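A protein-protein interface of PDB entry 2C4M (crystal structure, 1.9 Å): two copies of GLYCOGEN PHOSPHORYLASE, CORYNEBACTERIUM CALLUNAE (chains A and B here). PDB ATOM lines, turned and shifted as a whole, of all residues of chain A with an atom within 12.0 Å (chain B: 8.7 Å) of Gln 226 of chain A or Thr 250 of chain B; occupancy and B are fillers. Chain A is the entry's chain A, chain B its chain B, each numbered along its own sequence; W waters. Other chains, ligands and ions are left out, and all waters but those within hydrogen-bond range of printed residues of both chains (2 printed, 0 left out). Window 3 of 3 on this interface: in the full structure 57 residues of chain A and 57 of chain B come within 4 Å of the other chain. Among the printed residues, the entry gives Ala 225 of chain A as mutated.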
ATOM      1  N   PHE A 218      22.280  25.336  26.940  1.00  0.00           N
ATOM      2  CA  PHE A 218      21.498  24.536  26.026  1.00  0.00           C
ATOM      3  C   PHE A 218      21.227  25.402  24.814  1.00  0.00           C
ATOM      4  O   PHE A 218      21.534  26.590  24.834  1.00  0.00           O
ATOM      5  CB  PHE A 218      20.198  24.016  26.681  1.00  0.00           C
ATOM      6  CG  PHE A 218      19.244  25.092  27.149  1.00  0.00           C
ATOM      7  CD1 PHE A 218      18.326  25.670  26.270  1.00  0.00           C
ATOM      8  CD2 PHE A 218      19.232  25.493  28.482  1.00  0.00           C
ATOM      9  CE1 PHE A 218      17.402  26.632  26.720  1.00  0.00           C
ATOM     10  CE2 PHE A 218      18.318  26.451  28.945  1.00  0.00           C
ATOM     11  CZ  PHE A 218      17.400  27.022  28.063  1.00  0.00           C
ATOM     12  N   ASP A 219      20.721  24.795  23.751  1.00  0.00           N
ATOM     13  CA  ASP A 219      20.361  25.484  22.518  1.00  0.00           C
ATOM     14  C   ASP A 219      19.007  26.181  22.652  1.00  0.00           C
ATOM     15  O   ASP A 219      17.948  25.584  22.510  1.00  0.00           O
ATOM     16  CB  ASP A 219      20.306  24.447  21.392  1.00  0.00           C
ATOM     17  CG  ASP A 219      20.213  25.155  20.047  1.00  0.00           C
ATOM     18  OD1 ASP A 219      19.756  26.299  20.030  1.00  0.00           O
ATOM     19  OD2 ASP A 219      20.578  24.556  19.038  1.00  0.00           O
ATOM     20  N   TYR A 220      19.056  27.484  22.980  1.00  0.00           N
ATOM     21  CA  TYR A 220      17.803  28.169  23.287  1.00  0.00           C
ATOM     22  C   TYR A 220      16.872  28.235  22.069  1.00  0.00           C
ATOM     23  O   TYR A 220      15.656  28.145  22.180  1.00  0.00           O
ATOM     24  CB  TYR A 220      18.100  29.573  23.821  1.00  0.00           C
ATOM     25  CG  TYR A 220      16.820  30.231  24.205  1.00  0.00           C
ATOM     26  CD1 TYR A 220      16.115  30.980  23.267  1.00  0.00           C
ATOM     27  CD2 TYR A 220      16.321  30.099  25.501  1.00  0.00           C
ATOM     28  CE1 TYR A 220      14.916  31.584  23.619  1.00  0.00           C
ATOM     29  CE2 TYR A 220      15.127  30.711  25.855  1.00  0.00           C
ATOM     30  CZ  TYR A 220      14.429  31.455  24.921  1.00  0.00           C
ATOM     31  OH  TYR A 220      13.236  32.060  25.262  1.00  0.00           O
ATOM     32  N   ASP A 221      17.462  28.441  20.878  1.00  0.00           N
ATOM     33  CA  ASP A 221      16.625  28.516  19.683  1.00  0.00           C
ATOM     34  C   ASP A 221      15.852  27.213  19.450  1.00  0.00           C
ATOM     35  O   ASP A 221      14.682  27.209  19.090  1.00  0.00           O
ATOM     36  CB  ASP A 221      17.523  28.817  18.484  1.00  0.00           C
ATOM     37  CG  ASP A 221      17.950  30.279  18.524  1.00  0.00           C
ATOM     38  OD1 ASP A 221      17.399  31.014  19.344  1.00  0.00           O
ATOM     39  OD2 ASP A 221      18.821  30.661  17.748  1.00  0.00           O
ATOM     40  N   ALA A 222      16.567  26.057  19.607  1.00  0.00           N
ATOM     41  CA  ALA A 222      15.870  24.770  19.461  1.00  0.00           C
ATOM     42  C   ALA A 222      14.791  24.605  20.515  1.00  0.00           C
ATOM     43  O   ALA A 222      13.698  24.123  20.261  1.00  0.00           O
ATOM     44  CB  ALA A 222      16.849  23.594  19.560  1.00  0.00           C
ATOM     45  N   PHE A 223      15.171  24.909  21.766  1.00  0.00           N
ATOM     46  CA  PHE A 223      14.190  24.825  22.838  1.00  0.00           C
ATOM     47  C   PHE A 223      12.948  25.658  22.523  1.00  0.00           C
ATOM     48  O   PHE A 223      11.816  25.223  22.692  1.00  0.00           O
ATOM     49  CB  PHE A 223      14.844  25.330  24.125  1.00  0.00           C
ATOM     50  CG  PHE A 223      13.946  25.054  25.294  1.00  0.00           C
ATOM     51  CD1 PHE A 223      13.968  23.801  25.896  1.00  0.00           C
ATOM     52  CD2 PHE A 223      13.096  26.042  25.764  1.00  0.00           C
ATOM     53  CE1 PHE A 223      13.136  23.542  26.976  1.00  0.00           C
ATOM     54  CE2 PHE A 223      12.265  25.774  26.848  1.00  0.00           C
ATOM     55  CZ  PHE A 223      12.282  24.526  27.458  1.00  0.00           C
ATOM     56  N   ASN A 224      13.192  26.908  22.088  1.00  0.00           N
ATOM     57  CA  ASN A 224      12.092  27.833  21.807  1.00  0.00           C
ATOM     58  C   ASN A 224      11.235  27.347  20.631  1.00  0.00           C
ATOM     59  O   ASN A 224      10.039  27.600  20.536  1.00  0.00           O
ATOM     60  CB  ASN A 224      12.683  29.211  21.493  1.00  0.00           C
ATOM     61  CG  ASN A 224      11.592  30.257  21.446  1.00  0.00           C
ATOM     62  OD1 ASN A 224      10.921  30.539  22.437  1.00  0.00           O
ATOM     63  ND2 ASN A 224      11.367  30.796  20.236  1.00  0.00           N
ATOM     64  N   ALA A 225      11.875  26.567  19.746  1.00  0.00           N
ATOM     65  CA  ALA A 225      11.111  25.935  18.682  1.00  0.00           C
ATOM     66  C   ALA A 225      10.409  24.676  19.192  1.00  0.00           C
ATOM     67  O   ALA A 225       9.709  23.973  18.471  1.00  0.00           O
ATOM     68  CB  ALA A 225      12.078  25.582  17.551  1.00  0.00           C
ATOM     69  N   GLN A 226      10.661  24.394  20.488  1.00  0.00           N
ATOM     70  CA  GLN A 226      10.032  23.254  21.138  1.00  0.00           C
ATOM     71  C   GLN A 226      10.503  21.918  20.554  1.00  0.00           C
ATOM     72  O   GLN A 226       9.784  20.927  20.532  1.00  0.00           O
ATOM     73  CB  GLN A 226       8.516  23.399  21.016  1.00  0.00           C
ATOM     74  CG  GLN A 226       7.973  24.533  21.888  1.00  0.00           C
ATOM     75  CD  GLN A 226       6.838  25.225  21.170  1.00  0.00           C
ATOM     76  OE1 GLN A 226       5.750  24.701  20.992  1.00  0.00           O
ATOM     77  NE2 GLN A 226       7.165  26.435  20.673  1.00  0.00           N
ATOM     78  N   ARG A 227      11.707  21.944  19.979  1.00  0.00           N
ATOM     79  CA  ARG A 227      12.419  20.699  19.800  1.00  0.00           C
ATOM     80  C   ARG A 227      13.240  20.376  21.030  1.00  0.00           C
ATOM     81  O   ARG A 227      14.434  20.636  21.090  1.00  0.00           O
ATOM     82  CB  ARG A 227      13.337  20.832  18.583  1.00  0.00           C
ATOM     83  CG  ARG A 227      12.567  21.057  17.272  1.00  0.00           C
ATOM     84  CD  ARG A 227      13.509  21.129  16.059  1.00  0.00           C
ATOM     85  NE  ARG A 227      13.922  22.513  15.805  1.00  0.00           N
ATOM     86  CZ  ARG A 227      15.208  22.834  16.058  1.00  0.00           C
ATOM     87  NH1 ARG A 227      16.044  21.920  16.512  1.00  0.00           N
ATOM     88  NH2 ARG A 227      15.627  24.086  15.851  1.00  0.00           N
ATOM     89  N   PHE A 228      12.547  19.894  22.059  1.00  0.00           N
ATOM     90  CA  PHE A 228      13.130  19.722  23.384  1.00  0.00           C
ATOM     91  C   PHE A 228      14.342  18.820  23.509  1.00  0.00           C
ATOM     92  O   PHE A 228      15.259  19.132  24.261  1.00  0.00           O
ATOM     93  CB  PHE A 228      12.019  19.323  24.359  1.00  0.00           C
ATOM     94  CG  PHE A 228      10.923  20.369  24.477  1.00  0.00           C
ATOM     95  CD1 PHE A 228      11.235  21.713  24.646  1.00  0.00           C
ATOM     96  CD2 PHE A 228       9.584  20.000  24.418  1.00  0.00           C
ATOM     97  CE1 PHE A 228      10.223  22.675  24.755  1.00  0.00           C
ATOM     98  CE2 PHE A 228       8.568  20.954  24.526  1.00  0.00           C
ATOM     99  CZ  PHE A 228       8.890  22.289  24.694  1.00  0.00           C
ATOM    100  N   THR A 229      14.366  17.711  22.786  1.00  0.00           N
ATOM    101  CA  THR A 229      15.534  16.855  22.869  1.00  0.00           C
ATOM    102  C   THR A 229      16.697  17.520  22.119  1.00  0.00           C
ATOM    103  O   THR A 229      17.811  17.575  22.630  1.00  0.00           O
ATOM    104  CB  THR A 229      15.250  15.454  22.298  1.00  0.00           C
ATOM    105  OG1 THR A 229      14.309  14.780  23.145  1.00  0.00           O
ATOM    106  CG2 THR A 229      16.540  14.635  22.241  1.00  0.00           C
ATOM    107  N   ASP A 230      16.440  18.039  20.919  1.00  0.00           N
ATOM    108  CA  ASP A 230      17.476  18.709  20.140  1.00  0.00           C
ATOM    109  C   ASP A 230      18.163  19.803  20.970  1.00  0.00           C
ATOM    110  O   ASP A 230      19.341  20.106  20.807  1.00  0.00           O
ATOM    111  CB  ASP A 230      16.830  19.330  18.898  1.00  0.00           C
ATOM    112  CG  ASP A 230      16.565  18.274  17.824  1.00  0.00           C
ATOM    113  OD1 ASP A 230      16.794  17.094  18.094  1.00  0.00           O
ATOM    114  OD2 ASP A 230      16.087  18.636  16.749  1.00  0.00           O
ATOM    115  N   ALA A 231      17.358  20.458  21.842  1.00  0.00           N
ATOM    116  CA  ALA A 231      17.897  21.570  22.618  1.00  0.00           C
ATOM    117  C   ALA A 231      19.029  21.164  23.583  1.00  0.00           C
ATOM    118  O   ALA A 231      19.881  21.960  23.935  1.00  0.00           O
ATOM    119  CB  ALA A 231      16.750  22.228  23.384  1.00  0.00           C
ATOM    120  N   ILE A 232      18.980  19.908  24.078  1.00  0.00           N
ATOM    121  CA  ILE A 232      19.999  19.519  25.047  1.00  0.00           C
ATOM    122  C   ILE A 232      20.999  18.460  24.538  1.00  0.00           C
ATOM    123  O   ILE A 232      21.740  17.873  25.316  1.00  0.00           O
ATOM    124  CB  ILE A 232      19.309  19.009  26.317  1.00  0.00           C
ATOM    125  CG1 ILE A 232      18.235  17.974  25.978  1.00  0.00           C
ATOM    126  CG2 ILE A 232      18.628  20.174  27.058  1.00  0.00           C
ATOM    127  CD1 ILE A 232      18.826  16.638  25.520  1.00  0.00           C
ATOM    128  N   ILE A 233      21.006  18.171  23.213  1.00  0.00           N
ATOM    129  CA  ILE A 233      21.908  17.089  22.830  1.00  0.00           C
ATOM    130  C   ILE A 233      23.384  17.439  23.063  1.00  0.00           C
ATOM    131  O   ILE A 233      24.145  16.687  23.655  1.00  0.00           O
ATOM    132  CB  ILE A 233      21.657  16.739  21.361  1.00  0.00           C
ATOM    133  CG1 ILE A 233      20.454  15.798  21.262  1.00  0.00           C
ATOM    134  CG2 ILE A 233      22.877  16.001  20.780  1.00  0.00           C
ATOM    135  CD1 ILE A 233      19.798  15.827  19.881  1.00  0.00           C
ATOM    136  N   ASP B 240      12.963  19.445  31.800  1.00  0.00           N
ATOM    137  CA  ASP B 240      12.280  20.503  31.060  1.00  0.00           C
ATOM    138  C   ASP B 240      11.193  21.166  31.913  1.00  0.00           C
ATOM    139  O   ASP B 240      10.827  22.314  31.686  1.00  0.00           O
ATOM    140  CB  ASP B 240      11.682  19.930  29.778  1.00  0.00           C
ATOM    141  CG  ASP B 240      12.727  19.690  28.712  1.00  0.00           C
ATOM    142  OD1 ASP B 240      13.800  20.335  28.764  1.00  0.00           O
ATOM    143  OD2 ASP B 240      12.476  18.851  27.820  1.00  0.00           O
ATOM    144  N   TYR B 246       7.570  30.082  31.193  1.00  0.00           N
ATOM    145  CA  TYR B 246       6.839  30.505  30.007  1.00  0.00           C
ATOM    146  C   TYR B 246       7.512  29.994  28.731  1.00  0.00           C
ATOM    147  O   TYR B 246       7.819  30.772  27.822  1.00  0.00           O
ATOM    148  CB  TYR B 246       6.729  32.032  29.947  1.00  0.00           C
ATOM    149  CG  TYR B 246       5.745  32.627  30.936  1.00  0.00           C
ATOM    150  CD1 TYR B 246       6.043  32.691  32.290  1.00  0.00           C
ATOM    151  CD2 TYR B 246       4.512  33.122  30.510  1.00  0.00           C
ATOM    152  CE1 TYR B 246       5.145  33.235  33.205  1.00  0.00           C
ATOM    153  CE2 TYR B 246       3.601  33.668  31.421  1.00  0.00           C
ATOM    154  CZ  TYR B 246       3.932  33.721  32.767  1.00  0.00           C
ATOM    155  OH  TYR B 246       3.066  34.281  33.675  1.00  0.00           O
ATOM    156  N   PRO B 247       7.768  28.679  28.653  1.00  0.00           N
ATOM    157  CA  PRO B 247       8.404  28.138  27.450  1.00  0.00           C
ATOM    158  C   PRO B 247       7.450  28.334  26.276  1.00  0.00           C
ATOM    159  O   PRO B 247       6.236  28.177  26.429  1.00  0.00           O
ATOM    160  CB  PRO B 247       8.615  26.666  27.804  1.00  0.00           C
ATOM    161  CG  PRO B 247       7.496  26.376  28.749  1.00  0.00           C
ATOM    162  CD  PRO B 247       7.462  27.607  29.618  1.00  0.00           C
ATOM    163  N   ASN B 248       7.991  28.692  25.116  1.00  0.00           N
ATOM    164  CA  ASN B 248       7.169  28.915  23.929  1.00  0.00           C
ATOM    165  C   ASN B 248       6.197  27.750  23.724  1.00  0.00           C
ATOM    166  O   ASN B 248       6.581  26.586  23.805  1.00  0.00           O
ATOM    167  CB  ASN B 248       8.066  29.090  22.704  1.00  0.00           C
ATOM    168  CG  ASN B 248       7.350  29.762  21.543  1.00  0.00           C
ATOM    169  OD1 ASN B 248       6.231  30.255  21.689  1.00  0.00           O
ATOM    170  ND2 ASN B 248       7.998  29.798  20.389  1.00  0.00           N
ATOM    171  N   ASP B 249       4.931  28.062  23.468  1.00  0.00           N
ATOM    172  CA  ASP B 249       3.934  27.016  23.277  1.00  0.00           C
ATOM    173  C   ASP B 249       3.133  27.150  21.982  1.00  0.00           C
ATOM    174  O   ASP B 249       1.903  27.010  21.973  1.00  0.00           O
ATOM    175  CB  ASP B 249       2.972  26.986  24.466  1.00  0.00           C
ATOM    176  CG  ASP B 249       2.195  28.278  24.620  1.00  0.00           C
ATOM    177  OD1 ASP B 249       2.538  29.257  23.925  1.00  0.00           O
ATOM    178  OD2 ASP B 249       1.240  28.314  25.428  1.00  0.00           O
ATOM    179  N   THR B 250       3.832  27.406  20.882  1.00  0.00           N
ATOM    180  CA  THR B 250       3.166  27.535  19.594  1.00  0.00           C
ATOM    181  C   THR B 250       2.766  26.171  19.039  1.00  0.00           C
ATOM    182  O   THR B 250       1.981  26.097  18.103  1.00  0.00           O
ATOM    183  CB  THR B 250       4.068  28.243  18.571  1.00  0.00           C
ATOM    184  OG1 THR B 250       5.338  27.577  18.512  1.00  0.00           O
ATOM    185  CG2 THR B 250       4.273  29.698  18.958  1.00  0.00           C
ATOM    186  N   THR B 251       3.306  25.094  19.607  1.00  0.00           N
ATOM    187  CA  THR B 251       2.975  23.749  19.143  1.00  0.00           C
ATOM    188  C   THR B 251       2.352  22.972  20.286  1.00  0.00           C
ATOM    189  O   THR B 251       2.445  23.379  21.447  1.00  0.00           O
ATOM    190  CB  THR B 251       4.234  22.963  18.678  1.00  0.00           C
ATOM    191  OG1 THR B 251       5.025  22.601  19.821  1.00  0.00           O
ATOM    192  CG2 THR B 251       5.078  23.814  17.723  1.00  0.00           C
ATOM    193  N   TYR B 252       1.733  21.848  19.950  1.00  0.00           N
ATOM    194  CA  TYR B 252       1.096  20.982  20.935  1.00  0.00           C
ATOM    195  C   TYR B 252       2.061  20.588  22.061  1.00  0.00           C
ATOM    196  O   TYR B 252       1.697  20.607  23.235  1.00  0.00           O
ATOM    197  CB  TYR B 252       0.604  19.714  20.249  1.00  0.00           C
ATOM    198  CG  TYR B 252      -0.168  18.769  21.136  1.00  0.00           C
ATOM    199  CD1 TYR B 252      -1.517  18.995  21.412  1.00  0.00           C
ATOM    200  CD2 TYR B 252       0.437  17.639  21.683  1.00  0.00           C
ATOM    201  CE1 TYR B 252      -2.242  18.121  22.202  1.00  0.00           C
ATOM    202  CE2 TYR B 252      -0.281  16.755  22.480  1.00  0.00           C
ATOM    203  CZ  TYR B 252      -1.623  17.003  22.733  1.00  0.00           C
ATOM    204  OH  TYR B 252      -2.350  16.123  23.504  1.00  0.00           O
ATOM    205  N   GLU B 253       3.280  20.205  21.692  1.00  0.00           N
ATOM    206  CA  GLU B 253       4.273  19.794  22.684  1.00  0.00           C
ATOM    207  C   GLU B 253       4.664  20.914  23.623  1.00  0.00           C
ATOM    208  O   GLU B 253       4.906  20.675  24.803  1.00  0.00           O
ATOM    209  CB  GLU B 253       5.531  19.241  22.005  1.00  0.00           C
ATOM    210  CG  GLU B 253       5.358  17.849  21.417  1.00  0.00           C
ATOM    211  CD  GLU B 253       4.799  16.865  22.423  1.00  0.00           C
ATOM    212  OE1 GLU B 253       5.344  16.788  23.549  1.00  0.00           O
ATOM    213  OE2 GLU B 253       3.815  16.161  22.094  1.00  0.00           O
ATOM    214  N   GLY B 254       4.746  22.134  23.106  1.00  0.00           N
ATOM    215  CA  GLY B 254       5.095  23.253  23.961  1.00  0.00           C
ATOM    216  C   GLY B 254       3.949  23.509  24.935  1.00  0.00           C
ATOM    217  O   GLY B 254       4.164  23.861  26.107  1.00  0.00           O
ATOM    218  N   LYS B 255       2.722  23.327  24.450  1.00  0.00           N
ATOM    219  CA  LYS B 255       1.549  23.522  25.289  1.00  0.00           C
ATOM    220  C   LYS B 255       1.486  22.429  26.350  1.00  0.00           C
ATOM    221  O   LYS B 255       1.148  22.694  27.499  1.00  0.00           O
ATOM    222  CB  LYS B 255       0.277  23.494  24.434  1.00  0.00           C
ATOM    223  CG  LYS B 255       0.138  24.673  23.479  1.00  0.00           C
ATOM    224  CD  LYS B 255      -1.208  24.629  22.759  1.00  0.00           C
ATOM    225  CE  LYS B 255      -1.423  25.851  21.870  1.00  0.00           C
ATOM    226  NZ  LYS B 255      -0.414  25.981  20.785  1.00  0.00           N
ATOM    227  N   LYS B 256       1.810  21.199  25.963  1.00  0.00           N
ATOM    228  CA  LYS B 256       1.788  20.094  26.913  1.00  0.00           C
ATOM    229  C   LYS B 256       2.828  20.329  28.010  1.00  0.00           C
ATOM    230  O   LYS B 256       2.617  19.951  29.157  1.00  0.00           O
ATOM    231  CB  LYS B 256       2.067  18.760  26.214  1.00  0.00           C
ATOM    232  CG  LYS B 256       2.170  17.597  27.184  1.00  0.00           C
ATOM    233  CD  LYS B 256       2.468  16.272  26.510  1.00  0.00           C
ATOM    234  CE  LYS B 256       1.254  15.683  25.839  1.00  0.00           C
ATOM    235  NZ  LYS B 256       1.482  14.250  25.490  1.00  0.00           N
ATOM    236  N   LEU B 257       3.952  20.944  27.658  1.00  0.00           N
ATOM    237  CA  LEU B 257       4.967  21.238  28.652  1.00  0.00           C
ATOM    238  C   LEU B 257       4.485  22.275  29.634  1.00  0.00           C
ATOM    239  O   LEU B 257       4.703  22.175  30.835  1.00  0.00           O
ATOM    240  CB  LEU B 257       6.233  21.714  27.950  1.00  0.00           C
ATOM    241  CG  LEU B 257       7.305  22.217  28.928  1.00  0.00           C
ATOM    242  CD1 LEU B 257       7.672  21.173  29.993  1.00  0.00           C
ATOM    243  CD2 LEU B 257       8.606  22.595  28.222  1.00  0.00           C
ATOM    244  N   ARG B 258       3.804  23.315  29.124  1.00  0.00           N
ATOM    245  CA  ARG B 258       3.311  24.318  30.057  1.00  0.00           C
ATOM    246  C   ARG B 258       2.353  23.703  31.076  1.00  0.00           C
ATOM    247  O   ARG B 258       2.375  23.987  32.264  1.00  0.00           O
ATOM    248  CB  ARG B 258       2.597  25.403  29.263  1.00  0.00           C
ATOM    249  CG  ARG B 258       3.575  26.458  28.760  1.00  0.00           C
ATOM    250  CD  ARG B 258       2.899  27.797  28.453  1.00  0.00           C
ATOM    251  NE  ARG B 258       3.876  28.706  27.847  1.00  0.00           N
ATOM    252  CZ  ARG B 258       3.566  30.010  27.761  1.00  0.00           C
ATOM    253  NH1 ARG B 258       2.394  30.451  28.192  1.00  0.00           N
ATOM    254  NH2 ARG B 258       4.463  30.867  27.267  1.00  0.00           N
ATOM    255  N   TRP B 345      -7.050  24.903  27.014  1.00  0.00           N
ATOM    256  CA  TRP B 345      -6.216  23.784  26.607  1.00  0.00           C
ATOM    257  C   TRP B 345      -7.004  22.666  25.959  1.00  0.00           C
ATOM    258  O   TRP B 345      -8.121  22.364  26.379  1.00  0.00           O
ATOM    259  CB  TRP B 345      -5.477  23.190  27.815  1.00  0.00           C
ATOM    260  CG  TRP B 345      -4.671  24.158  28.595  1.00  0.00           C
ATOM    261  CD1 TRP B 345      -4.914  24.585  29.868  1.00  0.00           C
ATOM    262  CD2 TRP B 345      -3.455  24.792  28.182  1.00  0.00           C
ATOM    263  NE1 TRP B 345      -3.924  25.442  30.279  1.00  0.00           N
ATOM    264  CE2 TRP B 345      -3.013  25.587  29.264  1.00  0.00           C
ATOM    265  CE3 TRP B 345      -2.694  24.762  27.004  1.00  0.00           C
ATOM    266  CZ2 TRP B 345      -1.839  26.350  29.203  1.00  0.00           C
ATOM    267  CZ3 TRP B 345      -1.526  25.524  26.945  1.00  0.00           C
ATOM    268  CH2 TRP B 345      -1.112  26.307  28.040  1.00  0.00           C
ATOM    269  N   GLY B 567       9.293  35.443  19.425  1.00  0.00           N
ATOM    270  CA  GLY B 567       8.696  35.325  18.092  1.00  0.00           C
ATOM    271  C   GLY B 567       7.927  36.583  17.649  1.00  0.00           C
ATOM    272  O   GLY B 567       7.299  36.629  16.604  1.00  0.00           O
HETATM  273  O   HOH W   1      14.617  17.704  26.814  1.00  0.00           O
HETATM  274  O   HOH W   2      10.961  29.311  25.230  1.00  0.00           O
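The side-chain amide nitrogen of Asn 248 of chain B lies within hydrogen-bond range of the backbone carbonyl oxygen of Asn 224 of chain A (3.0 Å). O of Asn 248 of chain B lies close to NE2 of Gln 226 of chain A (3.2 Å). The side-chain amide nitrogen of Gln 226 of chain A sits at hydrogen-bond distance from the side-chain hydroxyl of Thr 250 of chain B, 3.1 Å away. OE1 of Gln 226 of chain A is in hydrogen-bond range of OG1 of Thr 251 of chain B. OE1 of Gln 226 of chain A lies close to N of Gly 254 of chain B (3.5 Å).
The backbone carbonyl oxygen (O) of Asn 224 of chain A is in hydrogen-bond range of the side-chain amide nitrogen (NE2) of Gln 226 of chain A (3.1 Å). O of Pro 247 of chain B lies within hydrogen-bond range of NE of Arg 258 of chain B (2.8 Å). The backbone carbonyl oxygen of Asp 249 of chain B is in hydrogen-bond range of the side-chain amino group of Lys 255 of chain B (2.8 Å). OD2 of Asp 249 of chain B lies within salt-bridge range of NE of Arg 258 of chain B (3.6 Å). OG1 of Thr 251 of chain B lies within hydrogen-bond range of N of Gly 254 of chain B, at 3.3 Å.
Among the printed residues, pairs that only touch across the chains: Phe 228 of chain A with Asp 240 of chain B (3.5 Å), Phe 228 of chain A with Leu 257 of chain B (3.6 Å), Phe 228 of chain A with Glu 253 of chain B (3.7 Å), Gln 226 of chain A with Asp 249 of chain B (3.7 Å), Phe 223 of chain A with Asp 240 of chain B (3.7 Å), Phe 223 of chain A with Pro 247 of chain B (3.9 Å) and Phe 228 of chain A with Gly 254 of chain B (3.98 Å).
Of the printed residues of chain B, Phe 223 of chain A touches Asp 240 (3.7 Å) and Pro 247 (3.9 Å). No residue of chain B comes within 4 Å of Ala 225 of chain A. Gln 226 of chain A touches just these residues of chain B: Asn 248 (3.0 Å), Asp 249 (3.7 Å), Thr 250 (3.1 Å), Thr 251 (2.5 Å) and Gly 254 (3.4 Å). Of the printed residues of chain B, Phe 228 of chain A touches Asp 240 (3.5 Å), Glu 253 (3.7 Å), Gly 254 (3.98 Å) and Leu 257 (3.6 Å). Printed residues of chain A within 4 Å of Asp 240 of chain B: Phe 223 (3.7 Å) and Phe 228 (3.5 Å). Tyr 246 of chain B touches none of the printed residues of chain A. Of chain A, only Asn 224 (3.0 Å) and Gln 226 (3.0 Å) come within 4 Å of Asn 248 of chain B. Asp 249 of chain B touches one residue of chain A. Thr 250 of chain B touches just one residue of chain A: Gln 226 (3.1 Å). Glu 253 of chain B touches just one residue of chain A: Phe 228. Of the printed residues of chain A, Gly 254 of chain B touches Gln 226 and Phe 228. Lys 255 of chain B touches none of the printed residues of chain A. Printed residues of chain A within 4 Å of Leu 257 of chain B: Phe 228 (3.6 Å).
Of the 16 printed residues of chain B, 9 touch a printed residue of chain A. Of the 16 printed residues of chain A, 4 touch a printed residue of chain B. Hydrophobic or aromatic side chains of chain A that line the printed part of chain B: Phe 223 and Phe 228. Along chain A the printed residues that touch a printed residue of chain B span positions 223 to 228. Among the printed residues, no Asp or Glu carboxylate lies within 4 Å of a Lys or Arg side-chain nitrogen of the other chain.
No position is printed for both chains.
Water W1 bridges OD2 of Asp 240 of chain B (2.6 Å) and O of Phe 228 of chain A (3.0 Å). Water W2 lies within hydrogen-bond range of N of Asn 248 of chain B (3.0 Å) and OD1 of Asn 224 of chain A (3.1 Å).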
